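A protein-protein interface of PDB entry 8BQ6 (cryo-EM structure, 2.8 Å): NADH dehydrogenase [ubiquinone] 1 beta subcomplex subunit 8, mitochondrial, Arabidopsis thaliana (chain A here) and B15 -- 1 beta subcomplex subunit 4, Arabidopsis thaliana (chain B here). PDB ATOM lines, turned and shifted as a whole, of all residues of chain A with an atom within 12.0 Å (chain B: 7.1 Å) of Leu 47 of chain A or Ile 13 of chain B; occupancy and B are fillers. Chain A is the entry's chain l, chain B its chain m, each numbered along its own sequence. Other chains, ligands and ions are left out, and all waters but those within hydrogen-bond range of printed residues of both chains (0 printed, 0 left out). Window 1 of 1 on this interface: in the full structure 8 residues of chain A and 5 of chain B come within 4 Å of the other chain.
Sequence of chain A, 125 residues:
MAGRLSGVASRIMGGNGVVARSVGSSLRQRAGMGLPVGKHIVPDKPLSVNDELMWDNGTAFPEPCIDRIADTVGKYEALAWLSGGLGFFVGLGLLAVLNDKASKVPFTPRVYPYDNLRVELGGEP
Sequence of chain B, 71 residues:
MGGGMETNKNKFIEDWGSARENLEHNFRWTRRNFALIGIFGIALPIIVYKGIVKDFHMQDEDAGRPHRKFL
The backbone carbonyl oxygen (O) of Pro 43 of chain A is in hydrogen-bond range of the side-chain amide nitrogen (ND2) of Asn 10 of chain B.
The indole nitrogen of Trp 16 of chain B lies within hydrogen-bond range of the backbone carbonyl oxygen of Ser 48 of chain A (3.1 Å).
OD1 of Asn 10 of chain B is in hydrogen-bond range of N of Phe 12 of chain B, at 2.8 Å.
The side-chain amide oxygen (OD1) of Asn 10 of chain B sits at hydrogen-bond distance from the backbone NH (N) of Ile 13 of chain B (2.8 Å).
Among the printed residues, merely in contact across the chains: Asp 44 of chain A with Phe 12 of chain B, Val 42 of chain A with Asn 10 of chain B, Pro 43 of chain A with Phe 12 of chain B, Glu 52 of chain A with Trp 16 of chain B, Lys 45 of chain A with Phe 12 of chain B, Pro 46 of chain A with Phe 12 of chain B, Leu 47 of chain A with Ile 13 of chain B, Leu 47 of chain A with Trp 16 of chain B and Pro 43 of chain A with Ile 13 of chain B.
Of the printed residues of chain B, Val 42 of chain A touches Asn 10 (3.2 Å).
Printed residues of chain B within 4 Å of Asp 44 of chain A: Phe 12 (3.2 Å).
Leu 47 of chain A touches two residues of chain B.
Of the printed residues of chain B, Ser 48 of chain A touches Trp 16 (3.1 Å).
Of the printed residues of chain B, Glu 52 of chain A touches Trp 16 (3.4 Å).
Asn 10 of chain B touches just these residues of chain A: Val 42 (3.2 Å) and Pro 43 (3.5 Å).
No residue of chain A comes within 4 Å of Lys 11 of chain B.
Phe 12 of chain B touches just these residues of chain A: Pro 43 (3.2 Å), Asp 44 (3.2 Å), Lys 45 (3.5 Å) and Pro 46 (3.6 Å).
No residue of chain A comes within 4 Å of Asp 15 of chain B.
Trp 16 of chain B touches just these residues of chain A: Leu 47, Ser 48 and Glu 52.
No residue of chain A comes within 4 Å of Gly 17 of chain B.
Printed residues of chain B that touch a printed residue of chain A: Asn 10, Phe 12, Ile 13 and Trp 16.
Hydrophobic or aromatic side chains of chain B within 4 Å of the printed part of chain A: Phe 12, Ile 13 and Trp 16.
Hydrophobic or aromatic side chains of chain A within 4 Å of the printed part of chain B: Val 42, Pro 43 and Leu 47.
Among the printed residues, 11 pairs touch across the chains.
Among the printed residues, no Asp or Glu carboxylate lies within 4 Å of a Lys or Arg side-chain nitrogen of the other chain.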
ATOM      1  N   LYS A  39     -30.163 -14.020  23.908  1.00  0.00           N
ATOM      2  CA  LYS A  39     -29.212 -14.898  23.228  1.00  0.00           C
ATOM      3  C   LYS A  39     -29.692 -15.077  21.797  1.00  0.00           C
ATOM      4  O   LYS A  39     -30.705 -15.743  21.564  1.00  0.00           O
ATOM      5  CB  LYS A  39     -29.085 -16.242  23.942  1.00  0.00           C
ATOM      6  CG  LYS A  39     -27.786 -16.992  23.619  1.00  0.00           C
ATOM      7  CD  LYS A  39     -27.936 -17.827  22.351  1.00  0.00           C
ATOM      8  CE  LYS A  39     -26.601 -18.110  21.684  1.00  0.00           C
ATOM      9  NZ  LYS A  39     -26.741 -19.120  20.593  1.00  0.00           N
ATOM     10  N   HIS A  40     -28.963 -14.495  20.848  1.00  0.00           N
ATOM     11  CA  HIS A  40     -29.369 -14.566  19.451  1.00  0.00           C
ATOM     12  C   HIS A  40     -29.237 -15.990  18.929  1.00  0.00           C
ATOM     13  O   HIS A  40     -28.226 -16.662  19.159  1.00  0.00           O
ATOM     14  CB  HIS A  40     -28.531 -13.602  18.613  1.00  0.00           C
ATOM     15  CG  HIS A  40     -27.094 -14.000  18.496  1.00  0.00           C
ATOM     16  ND1 HIS A  40     -26.563 -14.545  17.347  1.00  0.00           N
ATOM     17  CD2 HIS A  40     -26.082 -13.952  19.393  1.00  0.00           C
ATOM     18  CE1 HIS A  40     -25.282 -14.804  17.539  1.00  0.00           C
ATOM     19  NE2 HIS A  40     -24.965 -14.452  18.772  1.00  0.00           N
ATOM     20  N   ILE A  41     -30.263 -16.452  18.215  1.00  0.00           N
ATOM     21  CA  ILE A  41     -30.291 -17.843  17.788  1.00  0.00           C
ATOM     22  C   ILE A  41     -29.302 -18.043  16.650  1.00  0.00           C
ATOM     23  O   ILE A  41     -29.424 -17.432  15.579  1.00  0.00           O
ATOM     24  CB  ILE A  41     -31.704 -18.267  17.368  1.00  0.00           C
ATOM     25  CG1 ILE A  41     -32.769 -17.564  18.216  1.00  0.00           C
ATOM     26  CG2 ILE A  41     -31.844 -19.781  17.499  1.00  0.00           C
ATOM     27  CD1 ILE A  41     -32.685 -17.855  19.698  1.00  0.00           C
ATOM     28  N   VAL A  42     -28.315 -18.897  16.886  1.00  0.00           N
ATOM     29  CA  VAL A  42     -27.340 -19.280  15.871  1.00  0.00           C
ATOM     30  C   VAL A  42     -27.929 -20.448  15.085  1.00  0.00           C
ATOM     31  O   VAL A  42     -28.328 -21.449  15.701  1.00  0.00           O
ATOM     32  CB  VAL A  42     -26.004 -19.669  16.515  1.00  0.00           C
ATOM     33  CG1 VAL A  42     -25.176 -20.494  15.564  1.00  0.00           C
ATOM     34  CG2 VAL A  42     -25.250 -18.433  16.970  1.00  0.00           C
ATOM     35  N   PRO A  43     -28.005 -20.370  13.756  1.00  0.00           N
ATOM     36  CA  PRO A  43     -28.654 -21.442  12.991  1.00  0.00           C
ATOM     37  C   PRO A  43     -28.004 -22.799  13.222  1.00  0.00           C
ATOM     38  O   PRO A  43     -26.786 -22.912  13.383  1.00  0.00           O
ATOM     39  CB  PRO A  43     -28.492 -20.988  11.537  1.00  0.00           C
ATOM     40  CG  PRO A  43     -28.313 -19.514  11.619  1.00  0.00           C
ATOM     41  CD  PRO A  43     -27.564 -19.264  12.891  1.00  0.00           C
ATOM     42  N   ASP A  44     -28.845 -23.834  13.251  1.00  0.00           N
ATOM     43  CA  ASP A  44     -28.402 -25.218  13.322  1.00  0.00           C
ATOM     44  C   ASP A  44     -28.988 -26.076  12.212  1.00  0.00           C
ATOM     45  O   ASP A  44     -28.727 -27.284  12.179  1.00  0.00           O
ATOM     46  CB  ASP A  44     -28.765 -25.832  14.680  1.00  0.00           C
ATOM     47  CG  ASP A  44     -30.136 -25.408  15.159  1.00  0.00           C
ATOM     48  OD1 ASP A  44     -31.053 -25.297  14.318  1.00  0.00           O
ATOM     49  OD2 ASP A  44     -30.298 -25.194  16.378  1.00  0.00           O
ATOM     50  N   LYS A  45     -29.759 -25.448  11.320  1.00  0.00           N
ATOM     51  CA  LYS A  45     -30.359 -26.163  10.165  1.00  0.00           C
ATOM     52  C   LYS A  45     -29.973 -25.413   8.885  1.00  0.00           C
ATOM     53  O   LYS A  45     -29.958 -24.163   8.918  1.00  0.00           O
ATOM     54  CB  LYS A  45     -31.880 -26.232  10.325  1.00  0.00           C
ATOM     55  CG  LYS A  45     -32.370 -27.094  11.480  1.00  0.00           C
ATOM     56  CD  LYS A  45     -33.876 -27.111  11.612  1.00  0.00           C
ATOM     57  CE  LYS A  45     -34.360 -27.989  12.746  1.00  0.00           C
ATOM     58  NZ  LYS A  45     -35.836 -27.966  12.865  1.00  0.00           N
ATOM     59  N   PRO A  46     -29.646 -26.113   7.773  1.00  0.00           N
ATOM     60  CA  PRO A  46     -29.300 -25.464   6.499  1.00  0.00           C
ATOM     61  C   PRO A  46     -30.228 -24.290   6.154  1.00  0.00           C
ATOM     62  O   PRO A  46     -31.425 -24.503   6.041  1.00  0.00           O
ATOM     63  CB  PRO A  46     -29.482 -26.605   5.490  1.00  0.00           C
ATOM     64  CG  PRO A  46     -29.068 -27.830   6.270  1.00  0.00           C
ATOM     65  CD  PRO A  46     -29.567 -27.574   7.678  1.00  0.00           C
ATOM     66  N   LEU A  47     -29.657 -23.092   5.988  1.00  0.00           N
ATOM     67  CA  LEU A  47     -30.474 -21.879   5.709  1.00  0.00           C
ATOM     68  C   LEU A  47     -31.069 -21.951   4.301  1.00  0.00           C
ATOM     69  O   LEU A  47     -30.306 -22.218   3.348  1.00  0.00           O
ATOM     70  CB  LEU A  47     -29.585 -20.642   5.850  1.00  0.00           C
ATOM     71  CG  LEU A  47     -29.239 -20.232   7.279  1.00  0.00           C
ATOM     72  CD1 LEU A  47     -28.661 -18.829   7.291  1.00  0.00           C
ATOM     73  CD2 LEU A  47     -30.464 -20.307   8.176  1.00  0.00           C
ATOM     74  N   SER A  48     -32.374 -21.690   4.178  1.00  0.00           N
ATOM     75  CA  SER A  48     -33.048 -21.705   2.851  1.00  0.00           C
ATOM     76  C   SER A  48     -32.996 -20.317   2.201  1.00  0.00           C
ATOM     77  O   SER A  48     -32.475 -19.377   2.833  1.00  0.00           O
ATOM     78  CB  SER A  48     -34.469 -22.193   2.981  1.00  0.00           C
ATOM     79  OG  SER A  48     -35.297 -21.201   3.572  1.00  0.00           O
ATOM     80  N   VAL A  49     -33.547 -20.190   0.988  1.00  0.00           N
ATOM     81  CA  VAL A  49     -33.562 -18.880   0.272  1.00  0.00           C
ATOM     82  C   VAL A  49     -34.677 -18.029   0.893  1.00  0.00           C
ATOM     83  O   VAL A  49     -35.548 -18.597   1.592  1.00  0.00           O
ATOM     84  CB  VAL A  49     -33.755 -19.051  -1.246  1.00  0.00           C
ATOM     85  CG1 VAL A  49     -32.636 -19.886  -1.850  1.00  0.00           C
ATOM     86  CG2 VAL A  49     -35.107 -19.651  -1.592  1.00  0.00           C
ATOM     87  N   ASN A  50     -34.654 -16.719   0.647  1.00  0.00           N
ATOM     88  CA  ASN A  50     -35.708 -15.805   1.171  1.00  0.00           C
ATOM     89  C   ASN A  50     -35.643 -15.831   2.700  1.00  0.00           C
ATOM     90  O   ASN A  50     -36.703 -15.831   3.333  1.00  0.00           O
ATOM     91  CB  ASN A  50     -37.088 -16.112   0.571  1.00  0.00           C
ATOM     92  CG  ASN A  50     -37.046 -16.398  -0.916  1.00  0.00           C
ATOM     93  OD1 ASN A  50     -36.181 -15.900  -1.633  1.00  0.00           O
ATOM     94  ND2 ASN A  50     -37.974 -17.213  -1.390  1.00  0.00           N
ATOM     95  N   ASP A  51     -34.428 -15.859   3.249  1.00  0.00           N
ATOM     96  CA  ASP A  51     -34.232 -15.874   4.720  1.00  0.00           C
ATOM     97  C   ASP A  51     -33.805 -14.478   5.166  1.00  0.00           C
ATOM     98  O   ASP A  51     -34.077 -14.130   6.330  1.00  0.00           O
ATOM     99  CB  ASP A  51     -33.219 -16.945   5.123  1.00  0.00           C
ATOM    100  CG  ASP A  51     -33.160 -17.199   6.618  1.00  0.00           C
ATOM    101  OD1 ASP A  51     -34.238 -17.311   7.238  1.00  0.00           O
ATOM    102  OD2 ASP A  51     -32.039 -17.268   7.152  1.00  0.00           O
ATOM    103  N   GLU A  52     -33.172 -13.704   4.273  1.00  0.00           N
ATOM    104  CA  GLU A  52     -32.830 -12.337   4.640  1.00  0.00           C
ATOM    105  C   GLU A  52     -34.061 -11.509   4.979  1.00  0.00           C
ATOM    106  O   GLU A  52     -33.927 -10.458   5.614  1.00  0.00           O
ATOM    107  CB  GLU A  52     -32.086 -11.651   3.500  1.00  0.00           C
ATOM    108  CG  GLU A  52     -32.949 -11.519   2.270  1.00  0.00           C
ATOM    109  CD  GLU A  52     -32.502 -12.409   1.146  1.00  0.00           C
ATOM    110  OE1 GLU A  52     -32.464 -13.642   1.336  1.00  0.00           O
ATOM    111  OE2 GLU A  52     -32.217 -11.877   0.055  1.00  0.00           O
ATOM    112  N   LEU A  53     -35.248 -11.944   4.551  1.00  0.00           N
ATOM    113  CA  LEU A  53     -36.479 -11.201   4.774  1.00  0.00           C
ATOM    114  C   LEU A  53     -37.456 -11.913   5.696  1.00  0.00           C
ATOM    115  O   LEU A  53     -38.628 -11.522   5.748  1.00  0.00           O
ATOM    116  CB  LEU A  53     -37.182 -10.909   3.438  1.00  0.00           C
ATOM    117  CG  LEU A  53     -37.645 -12.104   2.599  1.00  0.00           C
ATOM    118  CD1 LEU A  53     -38.957 -12.681   3.106  1.00  0.00           C
ATOM    119  CD2 LEU A  53     -37.790 -11.683   1.158  1.00  0.00           C
ATOM    120  N   MET A  54     -37.022 -12.935   6.423  1.00  0.00           N
ATOM    121  CA  MET A  54     -37.961 -13.730   7.203  1.00  0.00           C
ATOM    122  C   MET A  54     -37.571 -13.810   8.674  1.00  0.00           C
ATOM    123  O   MET A  54     -38.190 -13.162   9.520  1.00  0.00           O
ATOM    124  CB  MET A  54     -38.081 -15.133   6.607  1.00  0.00           C
ATOM    125  CG  MET A  54     -39.232 -15.278   5.619  1.00  0.00           C
ATOM    126  SD  MET A  54     -40.619 -14.180   5.983  1.00  0.00           S
ATOM    127  CE  MET A  54     -41.687 -15.280   6.908  1.00  0.00           C
ATOM    128  N   LYS B   9     -17.031 -18.248  12.197  1.00  0.00           N
ATOM    129  CA  LYS B   9     -17.802 -18.673  11.041  1.00  0.00           C
ATOM    130  C   LYS B   9     -18.862 -19.688  11.435  1.00  0.00           C
ATOM    131  O   LYS B   9     -18.624 -20.583  12.250  1.00  0.00           O
ATOM    132  CB  LYS B   9     -16.879 -19.285   9.991  1.00  0.00           C
ATOM    133  CG  LYS B   9     -16.667 -18.439   8.760  1.00  0.00           C
ATOM    134  CD  LYS B   9     -15.972 -17.132   9.075  1.00  0.00           C
ATOM    135  CE  LYS B   9     -15.029 -16.747   7.946  1.00  0.00           C
ATOM    136  NZ  LYS B   9     -15.754 -16.302   6.723  1.00  0.00           N
ATOM    137  N   ASN B  10     -20.035 -19.546  10.835  1.00  0.00           N
ATOM    138  CA  ASN B  10     -21.112 -20.509  10.965  1.00  0.00           C
ATOM    139  C   ASN B  10     -21.215 -21.297   9.667  1.00  0.00           C
ATOM    140  O   ASN B  10     -21.268 -20.707   8.583  1.00  0.00           O
ATOM    141  CB  ASN B  10     -22.428 -19.803  11.280  1.00  0.00           C
ATOM    142  CG  ASN B  10     -23.573 -20.762  11.422  1.00  0.00           C
ATOM    143  OD1 ASN B  10     -24.164 -21.186  10.434  1.00  0.00           O
ATOM    144  ND2 ASN B  10     -23.887 -21.126  12.654  1.00  0.00           N
ATOM    145  N   LYS B  11     -21.229 -22.626   9.779  1.00  0.00           N
ATOM    146  CA  LYS B  11     -21.215 -23.466   8.586  1.00  0.00           C
ATOM    147  C   LYS B  11     -22.500 -23.311   7.781  1.00  0.00           C
ATOM    148  O   LYS B  11     -22.474 -23.326   6.545  1.00  0.00           O
ATOM    149  CB  LYS B  11     -20.991 -24.928   8.978  1.00  0.00           C
ATOM    150  CG  LYS B  11     -21.662 -25.943   8.064  1.00  0.00           C
ATOM    151  CD  LYS B  11     -21.608 -27.347   8.648  1.00  0.00           C
ATOM    152  CE  LYS B  11     -22.829 -27.649   9.488  1.00  0.00           C
ATOM    153  NZ  LYS B  11     -23.948 -28.086   8.614  1.00  0.00           N
ATOM    154  N   PHE B  12     -23.630 -23.144   8.473  1.00  0.00           N
ATOM    155  CA  PHE B  12     -24.945 -23.018   7.787  1.00  0.00           C
ATOM    156  C   PHE B  12     -25.045 -21.649   7.104  1.00  0.00           C
ATOM    157  O   PHE B  12     -25.581 -21.589   5.982  1.00  0.00           O
ATOM    158  CB  PHE B  12     -26.098 -23.223   8.773  1.00  0.00           C
ATOM    159  CG  PHE B  12     -25.941 -24.415   9.681  1.00  0.00           C
ATOM    160  CD1 PHE B  12     -26.467 -25.644   9.327  1.00  0.00           C
ATOM    161  CD2 PHE B  12     -25.256 -24.314  10.882  1.00  0.00           C
ATOM    162  CE1 PHE B  12     -26.324 -26.741  10.160  1.00  0.00           C
ATOM    163  CE2 PHE B  12     -25.101 -25.415  11.709  1.00  0.00           C
ATOM    164  CZ  PHE B  12     -25.637 -26.627  11.347  1.00  0.00           C
ATOM    165  N   ILE B  13     -24.554 -20.590   7.761  1.00  0.00           N
ATOM    166  CA  ILE B  13     -24.651 -19.255   7.176  1.00  0.00           C
ATOM    167  C   ILE B  13     -23.707 -19.130   5.987  1.00  0.00           C
ATOM    168  O   ILE B  13     -24.045 -18.517   4.967  1.00  0.00           O
ATOM    169  CB  ILE B  13     -24.386 -18.179   8.244  1.00  0.00           C
ATOM    170  CG1 ILE B  13     -25.594 -18.054   9.175  1.00  0.00           C
ATOM    171  CG2 ILE B  13     -24.119 -16.838   7.603  1.00  0.00           C
ATOM    172  CD1 ILE B  13     -25.385 -17.093  10.317  1.00  0.00           C
ATOM    173  N   GLU B  14     -22.515 -19.721   6.090  1.00  0.00           N
ATOM    174  CA  GLU B  14     -21.574 -19.697   4.975  1.00  0.00           C
ATOM    175  C   GLU B  14     -22.073 -20.520   3.793  1.00  0.00           C
ATOM    176  O   GLU B  14     -21.882 -20.129   2.635  1.00  0.00           O
ATOM    177  CB  GLU B  14     -20.206 -20.186   5.439  1.00  0.00           C
ATOM    178  CG  GLU B  14     -19.062 -19.756   4.540  1.00  0.00           C
ATOM    179  CD  GLU B  14     -18.391 -18.495   5.032  1.00  0.00           C
ATOM    180  OE1 GLU B  14     -17.969 -17.669   4.196  1.00  0.00           O
ATOM    181  OE2 GLU B  14     -18.329 -18.310   6.259  1.00  0.00           O
ATOM    182  N   ASP B  15     -22.697 -21.670   4.061  1.00  0.00           N
ATOM    183  CA  ASP B  15     -23.290 -22.464   2.987  1.00  0.00           C
ATOM    184  C   ASP B  15     -24.359 -21.677   2.253  1.00  0.00           C
ATOM    185  O   ASP B  15     -24.440 -21.712   1.018  1.00  0.00           O
ATOM    186  CB  ASP B  15     -23.891 -23.743   3.559  1.00  0.00           C
ATOM    187  CG  ASP B  15     -22.889 -24.857   3.654  1.00  0.00           C
ATOM    188  OD1 ASP B  15     -21.679 -24.564   3.602  1.00  0.00           O
ATOM    189  OD2 ASP B  15     -23.309 -26.024   3.786  1.00  0.00           O
ATOM    190  N   TRP B  16     -25.180 -20.943   3.011  1.00  0.00           N
ATOM    191  CA  TRP B  16     -26.188 -20.051   2.382  1.00  0.00           C
ATOM    192  C   TRP B  16     -25.448 -19.017   1.526  1.00  0.00           C
ATOM    193  O   TRP B  16     -25.929 -18.725   0.420  1.00  0.00           O
ATOM    194  CB  TRP B  16     -27.045 -19.390   3.465  1.00  0.00           C
ATOM    195  CG  TRP B  16     -28.164 -18.523   2.984  1.00  0.00           C
ATOM    196  CD1 TRP B  16     -29.133 -18.836   2.076  1.00  0.00           C
ATOM    197  CD2 TRP B  16     -28.451 -17.189   3.432  1.00  0.00           C
ATOM    198  NE1 TRP B  16     -29.992 -17.782   1.915  1.00  0.00           N
ATOM    199  CE2 TRP B  16     -29.601 -16.759   2.737  1.00  0.00           C
ATOM    200  CE3 TRP B  16     -27.844 -16.318   4.343  1.00  0.00           C
ATOM    201  CZ2 TRP B  16     -30.150 -15.494   2.928  1.00  0.00           C
ATOM    202  CZ3 TRP B  16     -28.391 -15.069   4.533  1.00  0.00           C
ATOM    203  CH2 TRP B  16     -29.529 -14.667   3.834  1.00  0.00           C
ATOM    204  N   GLY B  17     -24.305 -18.514   2.015  1.00  0.00           N
ATOM    205  CA  GLY B  17     -23.574 -17.516   1.250  1.00  0.00           C
ATOM    206  C   GLY B  17     -23.007 -18.062  -0.048  1.00  0.00           C
ATOM    207  O   GLY B  17     -23.074 -17.410  -1.092  1.00  0.00           O
ATOM    208  N   SER B  18     -22.434 -19.267   0.000  1.00  0.00           N
ATOM    209  CA  SER B  18     -21.833 -19.836  -1.202  1.00  0.00           C
ATOM    210  C   SER B  18     -22.885 -20.278  -2.211  1.00  0.00           C
ATOM    211  O   SER B  18     -22.644 -20.209  -3.422  1.00  0.00           O
ATOM    212  CB  SER B  18     -20.931 -21.013  -0.840  1.00  0.00           C
ATOM    213  OG  SER B  18     -21.571 -21.880   0.076  1.00  0.00           O
ATOM    214  N   ALA B  19     -24.040 -20.750  -1.743  1.00  0.00           N
ATOM    215  CA  ALA B  19     -25.085 -21.166  -2.671  1.00  0.00           C
ATOM    216  C   ALA B  19     -25.647 -19.971  -3.431  1.00  0.00           C
ATOM    217  O   ALA B  19     -26.132 -20.114  -4.559  1.00  0.00           O
ATOM    218  CB  ALA B  19     -26.194 -21.902  -1.923  1.00  0.00           C
